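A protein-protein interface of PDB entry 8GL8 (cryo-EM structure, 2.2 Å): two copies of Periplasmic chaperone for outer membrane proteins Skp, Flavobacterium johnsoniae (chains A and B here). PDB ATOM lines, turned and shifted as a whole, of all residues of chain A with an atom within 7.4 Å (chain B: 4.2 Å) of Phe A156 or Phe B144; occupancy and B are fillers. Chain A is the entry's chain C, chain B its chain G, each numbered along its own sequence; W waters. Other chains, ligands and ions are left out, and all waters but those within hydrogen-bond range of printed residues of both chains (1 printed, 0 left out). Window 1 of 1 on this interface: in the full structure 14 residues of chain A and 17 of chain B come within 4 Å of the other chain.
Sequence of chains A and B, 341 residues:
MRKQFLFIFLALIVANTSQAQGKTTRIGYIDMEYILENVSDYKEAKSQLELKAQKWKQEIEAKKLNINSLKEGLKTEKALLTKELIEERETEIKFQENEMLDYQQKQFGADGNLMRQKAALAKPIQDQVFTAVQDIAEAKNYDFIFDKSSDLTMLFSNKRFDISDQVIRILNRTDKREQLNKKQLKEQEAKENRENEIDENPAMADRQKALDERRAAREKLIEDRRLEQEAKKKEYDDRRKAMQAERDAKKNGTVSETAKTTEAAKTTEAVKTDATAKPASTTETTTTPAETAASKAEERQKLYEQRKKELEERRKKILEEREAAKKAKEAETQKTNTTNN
NE2 of Gln B134 sits at hydrogen-bond distance from O of Leu A155. The side-chain carboxylate of Asp B143 sits at hydrogen-bond distance from the side-chain amide nitrogen of Asn A158 (3.0 Å). The backbone carbonyl oxygen (O) of Ile B145 lies within hydrogen-bond range of the backbone NH (N) of Leu A155. O of Phe A156 sits at hydrogen-bond distance from N of Ile B145 (3.2 Å).
The backbone carbonyl oxygen (O) of Arg B26 lies within hydrogen-bond range of the backbone NH (N) of Asp B143. The backbone carbonyl oxygen (O) of Arg B26 lies within hydrogen-bond range of the backbone NH (N) of Phe B144, 3.3 Å away. The backbone NH (N) of Gly B28 is in hydrogen-bond range of the backbone carbonyl oxygen (O) of Phe B144 (2.8 Å). The backbone carbonyl oxygen (O) of Gly B28 lies within hydrogen-bond range of the backbone NH (N) of Phe B146 (3.0 Å). The side-chain hydroxyl (OH) of Tyr A29 lies close to the backbone NH (N) of Lys A159 (3.3 Å). The backbone NH of Tyr A29 lies within hydrogen-bond range of the backbone carbonyl oxygen of Phe A161, 3.3 Å away.
Ile A27 touches Ile B27. Ile A27 touches Phe B144 (O to CZ, 3.3 Å). Phe B144 touches Tyr A29. Thr A153 touches Phe B146. Met A154 touches Ile B145 (CA to O, 3.2 Å). Met A154 touches Phe B146. Gln B134 touches Phe A156. Phe A156 touches Ala B137 (CG to CB, 3.5 Å). O of Tyr B142 touches CE2 of Phe A156 (3.1 Å). Phe A161 touches Phe B144 (CD2 to CZ, 3.7 Å).
Phe A146 touches none of the printed residues of chain B. Lys A148 touches none of the printed residues of chain B. Of the printed residues of chain B, Thr A153 touches Phe B146. Of the printed residues of chain B, Met A154 touches Ile B145 and Phe B146. Of chain B, only Gln B134, Ala B137, Tyr B142, Asp B143, Phe B144 and Ile B145 come within 4 Å of Phe A156. Of the printed residues of chain B, Asn A158 touches Asp B143 (3.0 Å). Phe B144 touches five residues of chain A. Printed residues of chain A within 4 Å of Phe B146: Thr A153 (3.5 Å) and Met A154 (3.5 Å). The nearest printed residue of chain A that does not touch Ile B145 is Thr A153 (4.3 Å).
Of the 10 printed residues of chain B, 8 touch a printed residue of chain A. Hydrophobic or aromatic side chains of chain B within 4 Å of the printed part of chain A: Ile B27, Ala B137, Phe B144, Ile B145 and Phe B146. Of the 18 printed residues of chain A, 9 touch a printed residue of chain B. Printed residues of chain A that touch a printed residue of chain B: Ile A27, Tyr A29, Thr A153, Met A154, Leu A155, Phe A156, Ser A157, Asn A158 and Phe A161. Among the printed residues, no Asp or Glu carboxylate lies within 4 Å of a Lys or Arg side-chain nitrogen of the other chain.
Ile A27 touches its own counterpart, Ile B27. Ile A27 touches Phe B144, but with the chains exchanged Phe A144 does not touch Ile B27 (7.2 Å). Positions printed for both chains: 26, 27, 28, 142, 144 and 146. Of the 19 pairs that touch across the chains among the printed residues, 1 has its exchanged pair printed and touching as well.
Water W1 bridges NH1 of Arg A160 (3.2 Å) and OD1 of Asp B143 (3.4 Å).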
ATOM      1  N   ARG A  26      20.091 -20.885  -1.073  1.00  0.00           N
ATOM      2  CA  ARG A  26      20.121 -21.850  -2.161  1.00  0.00           C
ATOM      3  C   ARG A  26      20.260 -21.134  -3.496  1.00  0.00           C
ATOM      4  O   ARG A  26      19.712 -20.046  -3.691  1.00  0.00           O
ATOM      5  CB  ARG A  26      18.858 -22.711  -2.161  1.00  0.00           C
ATOM      6  CG  ARG A  26      18.372 -23.098  -0.780  1.00  0.00           C
ATOM      7  CD  ARG A  26      17.528 -24.354  -0.838  1.00  0.00           C
ATOM      8  NE  ARG A  26      18.020 -25.285  -1.844  1.00  0.00           N
ATOM      9  CZ  ARG A  26      17.247 -26.081  -2.569  1.00  0.00           C
ATOM     10  NH1 ARG A  26      15.931 -26.081  -2.429  1.00  0.00           N
ATOM     11  NH2 ARG A  26      17.807 -26.897  -3.458  1.00  0.00           N
ATOM     12  N   ILE A  27      20.999 -21.752  -4.413  1.00  0.00           N
ATOM     13  CA  ILE A  27      21.250 -21.196  -5.735  1.00  0.00           C
ATOM     14  C   ILE A  27      20.889 -22.243  -6.778  1.00  0.00           C
ATOM     15  O   ILE A  27      21.324 -23.394  -6.683  1.00  0.00           O
ATOM     16  CB  ILE A  27      22.716 -20.755  -5.899  1.00  0.00           C
ATOM     17  CG1 ILE A  27      23.064 -19.672  -4.879  1.00  0.00           C
ATOM     18  CG2 ILE A  27      22.971 -20.269  -7.312  1.00  0.00           C
ATOM     19  CD1 ILE A  27      24.366 -18.974  -5.156  1.00  0.00           C
ATOM     20  N   GLY A  28      20.088 -21.843  -7.766  1.00  0.00           N
ATOM     21  CA  GLY A  28      19.791 -22.672  -8.910  1.00  0.00           C
ATOM     22  C   GLY A  28      20.209 -21.968 -10.191  1.00  0.00           C
ATOM     23  O   GLY A  28      20.602 -20.799 -10.184  1.00  0.00           O
ATOM     24  N   TYR A  29      20.125 -22.699 -11.298  1.00  0.00           N
ATOM     25  CA  TYR A  29      20.465 -22.140 -12.596  1.00  0.00           C
ATOM     26  C   TYR A  29      19.444 -22.605 -13.623  1.00  0.00           C
ATOM     27  O   TYR A  29      18.737 -23.594 -13.423  1.00  0.00           O
ATOM     28  CB  TYR A  29      21.894 -22.502 -13.022  1.00  0.00           C
ATOM     29  CG  TYR A  29      22.205 -23.976 -13.074  1.00  0.00           C
ATOM     30  CD1 TYR A  29      22.490 -24.688 -11.919  1.00  0.00           C
ATOM     31  CD2 TYR A  29      22.242 -24.650 -14.282  1.00  0.00           C
ATOM     32  CE1 TYR A  29      22.785 -26.030 -11.967  1.00  0.00           C
ATOM     33  CE2 TYR A  29      22.537 -25.988 -14.339  1.00  0.00           C
ATOM     34  CZ  TYR A  29      22.809 -26.674 -13.180  1.00  0.00           C
ATOM     35  OH  TYR A  29      23.103 -28.013 -13.243  1.00  0.00           O
ATOM     36  N   TYR A 142      14.522 -21.021  -3.672  1.00  0.00           N
ATOM     37  CA  TYR A 142      15.782 -20.555  -4.231  1.00  0.00           C
ATOM     38  C   TYR A 142      15.929 -19.061  -3.993  1.00  0.00           C
ATOM     39  O   TYR A 142      14.980 -18.294  -4.174  1.00  0.00           O
ATOM     40  CB  TYR A 142      15.860 -20.853  -5.728  1.00  0.00           C
ATOM     41  CG  TYR A 142      16.132 -22.299  -6.060  1.00  0.00           C
ATOM     42  CD1 TYR A 142      17.257 -22.943  -5.574  1.00  0.00           C
ATOM     43  CD2 TYR A 142      15.268 -23.018  -6.869  1.00  0.00           C
ATOM     44  CE1 TYR A 142      17.510 -24.262  -5.878  1.00  0.00           C
ATOM     45  CE2 TYR A 142      15.513 -24.336  -7.179  1.00  0.00           C
ATOM     46  CZ  TYR A 142      16.634 -24.954  -6.681  1.00  0.00           C
ATOM     47  OH  TYR A 142      16.880 -26.270  -6.989  1.00  0.00           O
ATOM     48  N   PHE A 144      18.782 -17.269  -5.384  1.00  0.00           N
ATOM     49  CA  PHE A 144      19.321 -16.749  -6.628  1.00  0.00           C
ATOM     50  C   PHE A 144      19.110 -17.781  -7.723  1.00  0.00           C
ATOM     51  O   PHE A 144      19.157 -18.988  -7.474  1.00  0.00           O
ATOM     52  CB  PHE A 144      20.815 -16.414  -6.508  1.00  0.00           C
ATOM     53  CG  PHE A 144      21.156 -15.559  -5.318  1.00  0.00           C
ATOM     54  CD1 PHE A 144      21.467 -16.134  -4.100  1.00  0.00           C
ATOM     55  CD2 PHE A 144      21.157 -14.183  -5.417  1.00  0.00           C
ATOM     56  CE1 PHE A 144      21.779 -15.349  -3.008  1.00  0.00           C
ATOM     57  CE2 PHE A 144      21.470 -13.393  -4.332  1.00  0.00           C
ATOM     58  CZ  PHE A 144      21.779 -13.976  -3.126  1.00  0.00           C
ATOM     59  N   PHE A 146      20.782 -18.213 -11.351  1.00  0.00           N
ATOM     60  CA  PHE A 146      21.730 -17.784 -12.361  1.00  0.00           C
ATOM     61  C   PHE A 146      21.344 -18.347 -13.724  1.00  0.00           C
ATOM     62  O   PHE A 146      20.471 -19.206 -13.852  1.00  0.00           O
ATOM     63  CB  PHE A 146      23.143 -18.222 -11.990  1.00  0.00           C
ATOM     64  CG  PHE A 146      23.764 -17.410 -10.896  1.00  0.00           C
ATOM     65  CD1 PHE A 146      23.374 -17.580  -9.582  1.00  0.00           C
ATOM     66  CD2 PHE A 146      24.746 -16.480 -11.181  1.00  0.00           C
ATOM     67  CE1 PHE A 146      23.945 -16.836  -8.576  1.00  0.00           C
ATOM     68  CE2 PHE A 146      25.320 -15.734 -10.176  1.00  0.00           C
ATOM     69  CZ  PHE A 146      24.918 -15.912  -8.873  1.00  0.00           C
ATOM     70  N   LYS A 148      23.068 -20.281 -16.917  1.00  0.00           N
ATOM     71  CA  LYS A 148      24.263 -21.013 -17.315  1.00  0.00           C
ATOM     72  C   LYS A 148      24.763 -20.608 -18.693  1.00  0.00           C
ATOM     73  O   LYS A 148      25.924 -20.871 -19.018  1.00  0.00           O
ATOM     74  CB  LYS A 148      23.992 -22.517 -17.289  1.00  0.00           C
ATOM     75  CG  LYS A 148      24.832 -23.275 -16.283  1.00  0.00           C
ATOM     76  CD  LYS A 148      24.980 -24.734 -16.671  1.00  0.00           C
ATOM     77  CE  LYS A 148      26.442 -25.138 -16.748  1.00  0.00           C
ATOM     78  NZ  LYS A 148      26.724 -26.357 -15.941  1.00  0.00           N
ATOM     79  N   THR A 153      30.588 -17.977 -16.590  1.00  0.00           N
ATOM     80  CA  THR A 153      30.645 -19.409 -16.841  1.00  0.00           C
ATOM     81  C   THR A 153      30.848 -20.161 -15.534  1.00  0.00           C
ATOM     82  O   THR A 153      31.728 -19.813 -14.743  1.00  0.00           O
ATOM     83  CB  THR A 153      31.774 -19.752 -17.814  1.00  0.00           C
ATOM     84  OG1 THR A 153      32.998 -19.905 -17.090  1.00  0.00           O
ATOM     85  CG2 THR A 153      31.939 -18.653 -18.846  1.00  0.00           C
ATOM     86  N   MET A 154      30.029 -21.186 -15.313  1.00  0.00           N
ATOM     87  CA  MET A 154      30.216 -22.109 -14.204  1.00  0.00           C
ATOM     88  C   MET A 154      30.897 -23.359 -14.738  1.00  0.00           C
ATOM     89  O   MET A 154      30.311 -24.088 -15.543  1.00  0.00           O
ATOM     90  CB  MET A 154      28.890 -22.486 -13.547  1.00  0.00           C
ATOM     91  CG  MET A 154      27.780 -21.486 -13.715  1.00  0.00           C
ATOM     92  SD  MET A 154      26.214 -22.206 -13.195  1.00  0.00           S
ATOM     93  CE  MET A 154      25.149 -20.781 -13.314  1.00  0.00           C
ATOM     94  N   LEU A 155      32.125 -23.612 -14.288  1.00  0.00           N
ATOM     95  CA  LEU A 155      32.809 -24.826 -14.703  1.00  0.00           C
ATOM     96  C   LEU A 155      32.233 -26.063 -14.035  1.00  0.00           C
ATOM     97  O   LEU A 155      32.440 -27.174 -14.531  1.00  0.00           O
ATOM     98  CB  LEU A 155      34.302 -24.717 -14.404  1.00  0.00           C
ATOM     99  CG  LEU A 155      35.033 -23.568 -15.091  1.00  0.00           C
ATOM    100  CD1 LEU A 155      36.523 -23.782 -15.004  1.00  0.00           C
ATOM    101  CD2 LEU A 155      34.596 -23.458 -16.538  1.00  0.00           C
ATOM    102  N   PHE A 156      31.515 -25.897 -12.930  1.00  0.00           N
ATOM    103  CA  PHE A 156      30.886 -27.009 -12.238  1.00  0.00           C
ATOM    104  C   PHE A 156      29.516 -26.583 -11.738  1.00  0.00           C
ATOM    105  O   PHE A 156      29.351 -25.477 -11.218  1.00  0.00           O
ATOM    106  CB  PHE A 156      31.741 -27.495 -11.064  1.00  0.00           C
ATOM    107  CG  PHE A 156      31.169 -28.687 -10.360  1.00  0.00           C
ATOM    108  CD1 PHE A 156      31.353 -29.958 -10.869  1.00  0.00           C
ATOM    109  CD2 PHE A 156      30.439 -28.536  -9.198  1.00  0.00           C
ATOM    110  CE1 PHE A 156      30.824 -31.054 -10.229  1.00  0.00           C
ATOM    111  CE2 PHE A 156      29.907 -29.630  -8.555  1.00  0.00           C
ATOM    112  CZ  PHE A 156      30.099 -30.890  -9.070  1.00  0.00           C
ATOM    113  N   SER A 157      28.538 -27.468 -11.904  1.00  0.00           N
ATOM    114  CA  SER A 157      27.195 -27.269 -11.382  1.00  0.00           C
ATOM    115  C   SER A 157      26.716 -28.577 -10.774  1.00  0.00           C
ATOM    116  O   SER A 157      26.982 -29.653 -11.315  1.00  0.00           O
ATOM    117  CB  SER A 157      26.231 -26.805 -12.476  1.00  0.00           C
ATOM    118  OG  SER A 157      26.237 -25.394 -12.589  1.00  0.00           O
ATOM    119  N   ASN A 158      26.004 -28.481  -9.651  1.00  0.00           N
ATOM    120  CA  ASN A 158      25.618 -29.674  -8.908  1.00  0.00           C
ATOM    121  C   ASN A 158      24.568 -30.514  -9.624  1.00  0.00           C
ATOM    122  O   ASN A 158      24.315 -31.644  -9.192  1.00  0.00           O
ATOM    123  CB  ASN A 158      25.112 -29.283  -7.522  1.00  0.00           C
ATOM    124  CG  ASN A 158      25.213 -30.417  -6.527  1.00  0.00           C
ATOM    125  OD1 ASN A 158      26.080 -31.281  -6.643  1.00  0.00           O
ATOM    126  ND2 ASN A 158      24.336 -30.413  -5.534  1.00  0.00           N
ATOM    127  N   LYS A 159      23.930 -29.980 -10.664  1.00  0.00           N
ATOM    128  CA  LYS A 159      23.061 -30.732 -11.568  1.00  0.00           C
ATOM    129  C   LYS A 159      21.744 -31.133 -10.912  1.00  0.00           C
ATOM    130  O   LYS A 159      20.843 -31.639 -11.586  1.00  0.00           O
ATOM    131  CB  LYS A 159      23.782 -31.972 -12.109  1.00  0.00           C
ATOM    132  CG  LYS A 159      23.232 -32.485 -13.431  1.00  0.00           C
ATOM    133  CD  LYS A 159      24.345 -32.907 -14.374  1.00  0.00           C
ATOM    134  CE  LYS A 159      25.303 -33.879 -13.705  1.00  0.00           C
ATOM    135  NZ  LYS A 159      24.819 -35.284 -13.796  1.00  0.00           N
ATOM    136  N   ARG A 160      21.609 -30.901  -9.610  1.00  0.00           N
ATOM    137  CA  ARG A 160      20.329 -31.061  -8.938  1.00  0.00           C
ATOM    138  C   ARG A 160      19.692 -29.725  -8.602  1.00  0.00           C
ATOM    139  O   ARG A 160      18.565 -29.696  -8.099  1.00  0.00           O
ATOM    140  CB  ARG A 160      20.486 -31.903  -7.670  1.00  0.00           C
ATOM    141  CG  ARG A 160      21.420 -31.319  -6.638  1.00  0.00           C
ATOM    142  CD  ARG A 160      21.439 -32.174  -5.383  1.00  0.00           C
ATOM    143  NE  ARG A 160      20.414 -31.769  -4.431  1.00  0.00           N
ATOM    144  CZ  ARG A 160      20.659 -31.358  -3.195  1.00  0.00           C
ATOM    145  NH1 ARG A 160      21.892 -31.292  -2.720  1.00  0.00           N
ATOM    146  NH2 ARG A 160      19.642 -31.007  -2.414  1.00  0.00           N
ATOM    147  N   PHE A 161      20.391 -28.624  -8.865  1.00  0.00           N
ATOM    148  CA  PHE A 161      19.823 -27.287  -8.803  1.00  0.00           C
ATOM    149  C   PHE A 161      19.428 -26.772 -10.178  1.00  0.00           C
ATOM    150  O   PHE A 161      19.014 -25.617 -10.300  1.00  0.00           O
ATOM    151  CB  PHE A 161      20.808 -26.327  -8.142  1.00  0.00           C
ATOM    152  CG  PHE A 161      21.316 -26.805  -6.819  1.00  0.00           C
ATOM    153  CD1 PHE A 161      20.436 -27.147  -5.809  1.00  0.00           C
ATOM    154  CD2 PHE A 161      22.672 -26.915  -6.582  1.00  0.00           C
ATOM    155  CE1 PHE A 161      20.900 -27.588  -4.590  1.00  0.00           C
ATOM    156  CE2 PHE A 161      23.140 -27.355  -5.363  1.00  0.00           C
ATOM    157  CZ  PHE A 161      22.253 -27.693  -4.367  1.00  0.00           C
ATOM    158  N   ASP A 162      19.554 -27.600 -11.209  1.00  0.00           N
ATOM    159  CA  ASP A 162      19.121 -27.229 -12.549  1.00  0.00           C
ATOM    160  C   ASP A 162      17.607 -27.353 -12.633  1.00  0.00           C
ATOM    161  O   ASP A 162      17.059 -28.450 -12.483  1.00  0.00           O
ATOM    162  CB  ASP A 162      19.790 -28.115 -13.593  1.00  0.00           C
ATOM    163  CG  ASP A 162      19.557 -27.626 -15.007  1.00  0.00           C
ATOM    164  OD1 ASP A 162      19.020 -26.512 -15.173  1.00  0.00           O
ATOM    165  OD2 ASP A 162      19.910 -28.355 -15.956  1.00  0.00           O
ATOM    166  N   ARG B  26      27.911 -24.310  -1.287  1.00  0.00           N
ATOM    167  CA  ARG B  26      29.336 -24.016  -1.261  1.00  0.00           C
ATOM    168  C   ARG B  26      29.765 -23.593  -2.658  1.00  0.00           C
ATOM    169  O   ARG B  26      29.537 -24.322  -3.627  1.00  0.00           O
ATOM    170  CB  ARG B  26      30.140 -25.229  -0.795  1.00  0.00           C
ATOM    171  CG  ARG B  26      30.193 -25.395   0.710  1.00  0.00           C
ATOM    172  CD  ARG B  26      31.356 -26.274   1.122  1.00  0.00           C
ATOM    173  NE  ARG B  26      32.594 -25.515   1.243  1.00  0.00           N
ATOM    174  CZ  ARG B  26      33.783 -25.958   0.858  1.00  0.00           C
ATOM    175  NH1 ARG B  26      33.933 -27.155   0.316  1.00  0.00           N
ATOM    176  NH2 ARG B  26      34.848 -25.178   1.017  1.00  0.00           N
ATOM    177  N   ILE B  27      30.382 -22.420  -2.759  1.00  0.00           N
ATOM    178  CA  ILE B  27      30.778 -21.843  -4.036  1.00  0.00           C
ATOM    179  C   ILE B  27      32.290 -21.707  -4.066  1.00  0.00           C
ATOM    180  O   ILE B  27      32.889 -21.162  -3.132  1.00  0.00           O
ATOM    181  CB  ILE B  27      30.113 -20.476  -4.275  1.00  0.00           C
ATOM    182  CG1 ILE B  27      28.601 -20.578  -4.108  1.00  0.00           C
ATOM    183  CG2 ILE B  27      30.458 -19.953  -5.653  1.00  0.00           C
ATOM    184  CD1 ILE B  27      27.888 -19.303  -4.444  1.00  0.00           C
ATOM    185  N   GLY B  28      32.907 -22.213  -5.136  1.00  0.00           N
ATOM    186  CA  GLY B  28      34.303 -21.977  -5.410  1.00  0.00           C
ATOM    187  C   GLY B  28      34.444 -21.205  -6.712  1.00  0.00           C
ATOM    188  O   GLY B  28      33.463 -20.947  -7.415  1.00  0.00           O
ATOM    189  N   GLN B 134      36.493 -30.346 -12.201  1.00  0.00           N
ATOM    190  CA  GLN B 134      35.533 -31.411 -11.920  1.00  0.00           C
ATOM    191  C   GLN B 134      36.014 -32.277 -10.764  1.00  0.00           C
ATOM    192  O   GLN B 134      35.250 -32.585  -9.838  1.00  0.00           O
ATOM    193  CB  GLN B 134      35.302 -32.272 -13.164  1.00  0.00           C
ATOM    194  CG  GLN B 134      34.812 -31.530 -14.395  1.00  0.00           C
ATOM    195  CD  GLN B 134      33.665 -30.590 -14.104  1.00  0.00           C
ATOM    196  OE1 GLN B 134      32.543 -31.022 -13.845  1.00  0.00           O
ATOM    197  NE2 GLN B 134      33.939 -29.295 -14.155  1.00  0.00           N
ATOM    198  N   ALA B 137      35.877 -30.275  -7.389  1.00  0.00           N
ATOM    199  CA  ALA B 137      34.504 -30.116  -6.930  1.00  0.00           C
ATOM    200  C   ALA B 137      33.907 -31.439  -6.473  1.00  0.00           C
ATOM    201  O   ALA B 137      32.995 -31.448  -5.640  1.00  0.00           O
ATOM    202  CB  ALA B 137      33.651 -29.500  -8.035  1.00  0.00           C
ATOM    203  N   TYR B 142      31.852 -28.851  -3.329  1.00  0.00           N
ATOM    204  CA  TYR B 142      31.515 -27.581  -3.955  1.00  0.00           C
ATOM    205  C   TYR B 142      30.270 -27.765  -4.808  1.00  0.00           C
ATOM    206  O   TYR B 142      30.191 -28.706  -5.602  1.00  0.00           O
ATOM    207  CB  TYR B 142      32.666 -27.070  -4.820  1.00  0.00           C
ATOM    208  CG  TYR B 142      33.735 -26.323  -4.064  1.00  0.00           C
ATOM    209  CD1 TYR B 142      33.422 -25.223  -3.284  1.00  0.00           C
ATOM    210  CD2 TYR B 142      35.063 -26.714  -4.141  1.00  0.00           C
ATOM    211  CE1 TYR B 142      34.397 -24.537  -2.596  1.00  0.00           C
ATOM    212  CE2 TYR B 142      36.044 -26.034  -3.457  1.00  0.00           C
ATOM    213  CZ  TYR B 142      35.707 -24.947  -2.687  1.00  0.00           C
ATOM    214  OH  TYR B 142      36.685 -24.268  -2.003  1.00  0.00           O
ATOM    215  N   ASP B 143      29.299 -26.872  -4.640  1.00  0.00           N
ATOM    216  CA  ASP B 143      28.095 -26.923  -5.457  1.00  0.00           C
ATOM    217  C   ASP B 143      28.277 -26.204  -6.786  1.00  0.00           C
ATOM    218  O   ASP B 143      27.754 -26.656  -7.809  1.00  0.00           O
ATOM    219  CB  ASP B 143      26.915 -26.324  -4.691  1.00  0.00           C
ATOM    220  CG  ASP B 143      26.359 -27.272  -3.650  1.00  0.00           C
ATOM    221  OD1 ASP B 143      26.015 -28.416  -4.010  1.00  0.00           O
ATOM    222  OD2 ASP B 143      26.269 -26.876  -2.470  1.00  0.00           O
ATOM    223  N   PHE B 144      29.013 -25.095  -6.790  1.00  0.00           N
ATOM    224  CA  PHE B 144      29.265 -24.324  -7.996  1.00  0.00           C
ATOM    225  C   PHE B 144      30.724 -23.904  -8.033  1.00  0.00           C
ATOM    226  O   PHE B 144      31.303 -23.561  -7.000  1.00  0.00           O
ATOM    227  CB  PHE B 144      28.373 -23.079  -8.068  1.00  0.00           C
ATOM    228  CG  PHE B 144      26.908 -23.384  -8.114  1.00  0.00           C
ATOM    229  CD1 PHE B 144      26.267 -23.575  -9.322  1.00  0.00           C
ATOM    230  CD2 PHE B 144      26.170 -23.473  -6.948  1.00  0.00           C
ATOM    231  CE1 PHE B 144      24.920 -23.857  -9.366  1.00  0.00           C
ATOM    232  CE2 PHE B 144      24.824 -23.753  -6.988  1.00  0.00           C
ATOM    233  CZ  PHE B 144      24.199 -23.946  -8.198  1.00  0.00           C
ATOM    234  N   ILE B 145      31.313 -23.935  -9.225  1.00  0.00           N
ATOM    235  CA  ILE B 145      32.648 -23.400  -9.465  1.00  0.00           C
ATOM    236  C   ILE B 145      32.544 -22.434 -10.635  1.00  0.00           C
ATOM    237  O   ILE B 145      32.198 -22.842 -11.750  1.00  0.00           O
ATOM    238  CB  ILE B 145      33.677 -24.503  -9.763  1.00  0.00           C
ATOM    239  CG1 ILE B 145      33.733 -25.513  -8.614  1.00  0.00           C
ATOM    240  CG2 ILE B 145      35.045 -23.892 -10.029  1.00  0.00           C
ATOM    241  CD1 ILE B 145      34.726 -25.170  -7.534  1.00  0.00           C
ATOM    242  N   PHE B 146      32.841 -21.166 -10.386  1.00  0.00           N
ATOM    243  CA  PHE B 146      32.726 -20.121 -11.390  1.00  0.00           C
ATOM    244  C   PHE B 146      34.095 -19.762 -11.949  1.00  0.00           C
ATOM    245  O   PHE B 146      35.123 -19.961 -11.301  1.00  0.00           O
ATOM    246  CB  PHE B 146      32.078 -18.866 -10.802  1.00  0.00           C
ATOM    247  CG  PHE B 146      30.639 -19.042 -10.422  1.00  0.00           C
ATOM    248  CD1 PHE B 146      29.664 -19.164 -11.391  1.00  0.00           C
ATOM    249  CD2 PHE B 146      30.261 -19.076  -9.095  1.00  0.00           C
ATOM    250  CE1 PHE B 146      28.341 -19.320 -11.042  1.00  0.00           C
ATOM    251  CE2 PHE B 146      28.941 -19.232  -8.742  1.00  0.00           C
ATOM    252  CZ  PHE B 146      27.980 -19.355  -9.716  1.00  0.00           C
HETATM  253  O   HOH W   1      25.024 -30.947  -1.987  1.00  0.00           O
